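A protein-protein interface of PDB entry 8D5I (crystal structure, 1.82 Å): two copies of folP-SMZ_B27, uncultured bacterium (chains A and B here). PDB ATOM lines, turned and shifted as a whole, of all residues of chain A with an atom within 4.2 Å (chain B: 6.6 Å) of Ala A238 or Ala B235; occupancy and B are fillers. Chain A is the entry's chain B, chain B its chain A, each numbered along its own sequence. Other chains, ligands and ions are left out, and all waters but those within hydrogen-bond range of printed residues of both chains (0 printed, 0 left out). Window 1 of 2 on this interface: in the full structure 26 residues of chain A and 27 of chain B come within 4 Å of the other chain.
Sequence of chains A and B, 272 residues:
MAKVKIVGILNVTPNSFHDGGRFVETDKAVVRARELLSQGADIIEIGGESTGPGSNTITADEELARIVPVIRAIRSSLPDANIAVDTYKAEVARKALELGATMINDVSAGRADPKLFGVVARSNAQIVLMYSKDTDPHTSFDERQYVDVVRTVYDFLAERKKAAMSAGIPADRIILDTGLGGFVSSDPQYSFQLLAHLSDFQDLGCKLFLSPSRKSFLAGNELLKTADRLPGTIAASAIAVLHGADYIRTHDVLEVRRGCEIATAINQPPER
Pro B231 touches Ile A234 (O to CG2, 3.6 Å).
Ile A234 touches Ile B234.
Ala B238 touches Ala A235.
Ala A238 touches Ala B235 (CB to CB, 3.6 Å).
Ile B239 touches Leu A242.
CA of Gly A259 touches O of Pro B231 (3.95 Å).
O of Gly A259 touches CB of Ala B235, at 3.4 Å.
Ala A263 touches Ile B239.
Ile B234 touches its own counterpart, Ile A234.
Ala A235 touches Ala B238, and with the chains exchanged Ala A238 touches Ala B235.
Hydrophobic or aromatic side chains of chain A that line the printed part of chain B: Ile A234, Ala A235, Ala A238, Leu A242 and Ala A263.
Along chain B the printed residues that touch a printed residue of chain A span positions 231 to 239.
Among the printed residues, 8 pairs touch across the chains.
Among the printed residues, no Asp or Glu carboxylate lies within 4 Å of a Lys or Arg side-chain nitrogen of the other chain.
Of the printed residues of chain B, Ala A235 touches Ala B238 (3.7 Å).
Ala A236 touches none of the printed residues of chain B.
Ala A238 touches just one residue of chain B: Ala B235.
Of the printed residues of chain B, Gly A259 touches Pro B231 (3.95 Å) and Ala B235 (3.4 Å).
Of the printed residues of chain A, Pro B231 touches Ile A234 and Gly A259.
Gly B232 touches none of the printed residues of chain A.
Ala B235 touches two residues of chain A.
Printed residues of chain A within 4 Å of Ala B238: Ala A235.
The nearest residue of chain B that does not touch Ala A238 is Ile B239 (4.3 Å).
The nearest printed residue of chain B that does not touch Ala A235 is Ile B234 (4.3 Å).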
ATOM      1  N   ILE A 234       8.021 -30.212  -9.578  1.00  0.00           N
ATOM      2  CA  ILE A 234       7.611 -30.097  -8.182  1.00  0.00           C
ATOM      3  C   ILE A 234       8.113 -28.779  -7.591  1.00  0.00           C
ATOM      4  O   ILE A 234       7.361 -28.051  -6.931  1.00  0.00           O
ATOM      5  CB  ILE A 234       8.129 -31.302  -7.376  1.00  0.00           C
ATOM      6  CG1 ILE A 234       7.452 -32.596  -7.853  1.00  0.00           C
ATOM      7  CG2 ILE A 234       7.890 -31.071  -5.875  1.00  0.00           C
ATOM      8  CD1 ILE A 234       8.084 -33.854  -7.243  1.00  0.00           C
ATOM      9  N   ALA A 235       9.389 -28.448  -7.833  1.00  0.00           N
ATOM     10  CA  ALA A 235       9.941 -27.210  -7.281  1.00  0.00           C
ATOM     11  C   ALA A 235       9.219 -25.993  -7.847  1.00  0.00           C
ATOM     12  O   ALA A 235       8.859 -25.072  -7.101  1.00  0.00           O
ATOM     13  CB  ALA A 235      11.439 -27.111  -7.573  1.00  0.00           C
ATOM     14  N   ALA A 236       9.016 -25.964  -9.179  1.00  0.00           N
ATOM     15  CA  ALA A 236       8.380 -24.812  -9.817  1.00  0.00           C
ATOM     16  C   ALA A 236       6.934 -24.658  -9.373  1.00  0.00           C
ATOM     17  O   ALA A 236       6.460 -23.533  -9.158  1.00  0.00           O
ATOM     18  CB  ALA A 236       8.462 -24.924 -11.347  1.00  0.00           C
ATOM     19  N   SER A 237       6.220 -25.777  -9.225  1.00  0.00           N
ATOM     20  CA  SER A 237       4.817 -25.718  -8.820  1.00  0.00           C
ATOM     21  C   SER A 237       4.681 -25.295  -7.365  1.00  0.00           C
ATOM     22  O   SER A 237       3.750 -24.553  -7.014  1.00  0.00           O
ATOM     23  CB  SER A 237       4.134 -27.076  -9.040  1.00  0.00           C
ATOM     24  OG  SER A 237       4.136 -27.486 -10.410  1.00  0.00           O
ATOM     25  N   ALA A 238       5.585 -25.773  -6.499  1.00  0.00           N
ATOM     26  CA  ALA A 238       5.564 -25.351  -5.100  1.00  0.00           C
ATOM     27  C   ALA A 238       5.851 -23.862  -4.978  1.00  0.00           C
ATOM     28  O   ALA A 238       5.180 -23.147  -4.222  1.00  0.00           O
ATOM     29  CB  ALA A 238       6.580 -26.158  -4.286  1.00  0.00           C
ATOM     30  N   ILE A 239       6.838 -23.367  -5.727  1.00  0.00           N
ATOM     31  CA  ILE A 239       7.156 -21.947  -5.659  1.00  0.00           C
ATOM     32  C   ILE A 239       6.023 -21.100  -6.240  1.00  0.00           C
ATOM     33  O   ILE A 239       5.726 -20.008  -5.733  1.00  0.00           O
ATOM     34  CB  ILE A 239       8.504 -21.696  -6.357  1.00  0.00           C
ATOM     35  CG1 ILE A 239       9.622 -22.284  -5.504  1.00  0.00           C
ATOM     36  CG2 ILE A 239       8.770 -20.198  -6.500  1.00  0.00           C
ATOM     37  CD1 ILE A 239      10.953 -22.233  -6.157  1.00  0.00           C
ATOM     38  N   ALA A 240       5.355 -21.587  -7.287  1.00  0.00           N
ATOM     39  CA  ALA A 240       4.174 -20.890  -7.787  1.00  0.00           C
ATOM     40  C   ALA A 240       3.102 -20.784  -6.708  1.00  0.00           C
ATOM     41  O   ALA A 240       2.460 -19.732  -6.553  1.00  0.00           O
ATOM     42  CB  ALA A 240       3.623 -21.603  -9.027  1.00  0.00           C
ATOM     43  N   VAL A 241       2.892 -21.858  -5.947  1.00  0.00           N
ATOM     44  CA  VAL A 241       1.880 -21.804  -4.893  1.00  0.00           C
ATOM     45  C   VAL A 241       2.319 -20.832  -3.800  1.00  0.00           C
ATOM     46  O   VAL A 241       1.522 -20.015  -3.316  1.00  0.00           O
ATOM     47  CB  VAL A 241       1.616 -23.216  -4.341  1.00  0.00           C
ATOM     48  CG1 VAL A 241       0.944 -23.156  -2.972  1.00  0.00           C
ATOM     49  CG2 VAL A 241       0.779 -24.030  -5.344  1.00  0.00           C
ATOM     50  N   LEU A 242       3.606 -20.882  -3.422  1.00  0.00           N
ATOM     51  CA  LEU A 242       4.167 -19.945  -2.448  1.00  0.00           C
ATOM     52  C   LEU A 242       3.933 -18.496  -2.847  1.00  0.00           C
ATOM     53  O   LEU A 242       3.777 -17.625  -1.979  1.00  0.00           O
ATOM     54  CB  LEU A 242       5.664 -20.193  -2.313  1.00  0.00           C
ATOM     55  CG  LEU A 242       6.379 -19.513  -1.134  1.00  0.00           C
ATOM     56  CD1 LEU A 242       5.995 -20.188   0.170  1.00  0.00           C
ATOM     57  CD2 LEU A 242       7.885 -19.530  -1.344  1.00  0.00           C
ATOM     58  N   GLY A 259       3.983 -31.923  -2.934  1.00  0.00           N
ATOM     59  CA  GLY A 259       4.909 -30.806  -2.914  1.00  0.00           C
ATOM     60  C   GLY A 259       4.220 -29.480  -2.645  1.00  0.00           C
ATOM     61  O   GLY A 259       4.707 -28.665  -1.866  1.00  0.00           O
ATOM     62  N   CYS A 260       3.083 -29.235  -3.301  1.00  0.00           N
ATOM     63  CA  CYS A 260       2.410 -27.947  -3.149  1.00  0.00           C
ATOM     64  C   CYS A 260       1.779 -27.796  -1.771  1.00  0.00           C
ATOM     65  O   CYS A 260       1.573 -26.669  -1.309  1.00  0.00           O
ATOM     66  CB  CYS A 260       1.349 -27.789  -4.245  1.00  0.00           C
ATOM     67  SG  CYS A 260       2.074 -27.569  -5.909  1.00  0.00           S
ATOM     68  N   ALA A 263       4.329 -25.999   0.253  1.00  0.00           N
ATOM     69  CA  ALA A 263       4.314 -24.570  -0.045  1.00  0.00           C
ATOM     70  C   ALA A 263       3.160 -23.867   0.662  1.00  0.00           C
ATOM     71  O   ALA A 263       3.335 -22.775   1.213  1.00  0.00           O
ATOM     72  CB  ALA A 263       4.228 -24.355  -1.560  1.00  0.00           C
ATOM     73  N   LEU B 230       9.528 -37.736  -0.451  1.00  0.00           N
ATOM     74  CA  LEU B 230      10.441 -37.113  -1.409  1.00  0.00           C
ATOM     75  C   LEU B 230       9.848 -35.864  -2.054  1.00  0.00           C
ATOM     76  O   LEU B 230      10.553 -34.842  -2.109  1.00  0.00           O
ATOM     77  CB  LEU B 230      10.892 -38.119  -2.475  1.00  0.00           C
ATOM     78  CG  LEU B 230      11.809 -37.512  -3.553  1.00  0.00           C
ATOM     79  CD1 LEU B 230      13.028 -36.825  -2.929  1.00  0.00           C
ATOM     80  CD2 LEU B 230      12.253 -38.584  -4.525  1.00  0.00           C
ATOM     81  N   PRO B 231       8.607 -35.863  -2.569  1.00  0.00           N
ATOM     82  CA  PRO B 231       8.071 -34.603  -3.123  1.00  0.00           C
ATOM     83  C   PRO B 231       8.114 -33.447  -2.143  1.00  0.00           C
ATOM     84  O   PRO B 231       8.527 -32.343  -2.526  1.00  0.00           O
ATOM     85  CB  PRO B 231       6.632 -34.970  -3.531  1.00  0.00           C
ATOM     86  CG  PRO B 231       6.653 -36.462  -3.721  1.00  0.00           C
ATOM     87  CD  PRO B 231       7.620 -36.955  -2.656  1.00  0.00           C
ATOM     88  N   GLY B 232       7.711 -33.664  -0.886  1.00  0.00           N
ATOM     89  CA  GLY B 232       7.789 -32.594   0.093  1.00  0.00           C
ATOM     90  C   GLY B 232       9.206 -32.129   0.358  1.00  0.00           C
ATOM     91  O   GLY B 232       9.439 -30.938   0.576  1.00  0.00           O
ATOM     92  N   THR B 233      10.171 -33.061   0.342  1.00  0.00           N
ATOM     93  CA  THR B 233      11.578 -32.704   0.519  1.00  0.00           C
ATOM     94  C   THR B 233      12.075 -31.832  -0.629  1.00  0.00           C
ATOM     95  O   THR B 233      12.843 -30.890  -0.408  1.00  0.00           O
ATOM     96  CB  THR B 233      12.442 -33.970   0.611  1.00  0.00           C
ATOM     97  OG1 THR B 233      12.032 -34.756   1.742  1.00  0.00           O
ATOM     98  CG2 THR B 233      13.931 -33.597   0.817  1.00  0.00           C
ATOM     99  N   ILE B 234      11.680 -32.158  -1.866  1.00  0.00           N
ATOM    100  CA  ILE B 234      12.069 -31.339  -3.016  1.00  0.00           C
ATOM    101  C   ILE B 234      11.508 -29.928  -2.870  1.00  0.00           C
ATOM    102  O   ILE B 234      12.227 -28.935  -3.042  1.00  0.00           O
ATOM    103  CB  ILE B 234      11.603 -31.990  -4.334  1.00  0.00           C
ATOM    104  CG1 ILE B 234      12.278 -33.356  -4.551  1.00  0.00           C
ATOM    105  CG2 ILE B 234      11.842 -31.054  -5.515  1.00  0.00           C
ATOM    106  CD1 ILE B 234      11.667 -34.150  -5.688  1.00  0.00           C
ATOM    107  N   ALA B 235      10.211 -29.825  -2.541  1.00  0.00           N
ATOM    108  CA  ALA B 235       9.584 -28.517  -2.368  1.00  0.00           C
ATOM    109  C   ALA B 235      10.198 -27.716  -1.215  1.00  0.00           C
ATOM    110  O   ALA B 235      10.390 -26.498  -1.336  1.00  0.00           O
ATOM    111  CB  ALA B 235       8.087 -28.689  -2.148  1.00  0.00           C
ATOM    112  N   ALA B 236      10.454 -28.354  -0.066  1.00  0.00           N
ATOM    113  CA  ALA B 236      11.002 -27.603   1.065  1.00  0.00           C
ATOM    114  C   ALA B 236      12.434 -27.165   0.780  1.00  0.00           C
ATOM    115  O   ALA B 236      12.834 -26.043   1.132  1.00  0.00           O
ATOM    116  CB  ALA B 236      10.947 -28.434   2.359  1.00  0.00           C
ATOM    117  N   SER B 237      13.217 -28.041   0.146  1.00  0.00           N
ATOM    118  CA  SER B 237      14.600 -27.705  -0.184  1.00  0.00           C
ATOM    119  C   SER B 237      14.649 -26.595  -1.222  1.00  0.00           C
ATOM    120  O   SER B 237      15.468 -25.672  -1.111  1.00  0.00           O
ATOM    121  CB  SER B 237      15.339 -28.945  -0.693  1.00  0.00           C
ATOM    122  OG  SER B 237      15.396 -29.942   0.319  1.00  0.00           O
ATOM    123  N   ALA B 238      13.799 -26.688  -2.256  1.00  0.00           N
ATOM    124  CA  ALA B 238      13.716 -25.620  -3.244  1.00  0.00           C
ATOM    125  C   ALA B 238      13.349 -24.296  -2.588  1.00  0.00           C
ATOM    126  O   ALA B 238      13.926 -23.249  -2.910  1.00  0.00           O
ATOM    127  CB  ALA B 238      12.695 -25.978  -4.331  1.00  0.00           C
ATOM    128  N   ILE B 239      12.370 -24.310  -1.687  1.00  0.00           N
ATOM    129  CA  ILE B 239      11.933 -23.045  -1.106  1.00  0.00           C
ATOM    130  C   ILE B 239      13.013 -22.495  -0.166  1.00  0.00           C
ATOM    131  O   ILE B 239      13.250 -21.282  -0.122  1.00  0.00           O
ATOM    132  CB  ILE B 239      10.562 -23.225  -0.425  1.00  0.00           C
ATOM    133  CG1 ILE B 239       9.481 -23.346  -1.526  1.00  0.00           C
ATOM    134  CG2 ILE B 239      10.228 -22.062   0.517  1.00  0.00           C
ATOM    135  CD1 ILE B 239       8.120 -23.796  -1.029  1.00  0.00           C
ATOM    136  N   ALA B 240      13.719 -23.377   0.544  1.00  0.00           N
ATOM    137  CA  ALA B 240      14.859 -22.944   1.357  1.00  0.00           C
ATOM    138  C   ALA B 240      15.920 -22.240   0.509  1.00  0.00           C
ATOM    139  O   ALA B 240      16.442 -21.182   0.896  1.00  0.00           O
ATOM    140  CB  ALA B 240      15.466 -24.143   2.093  1.00  0.00           C
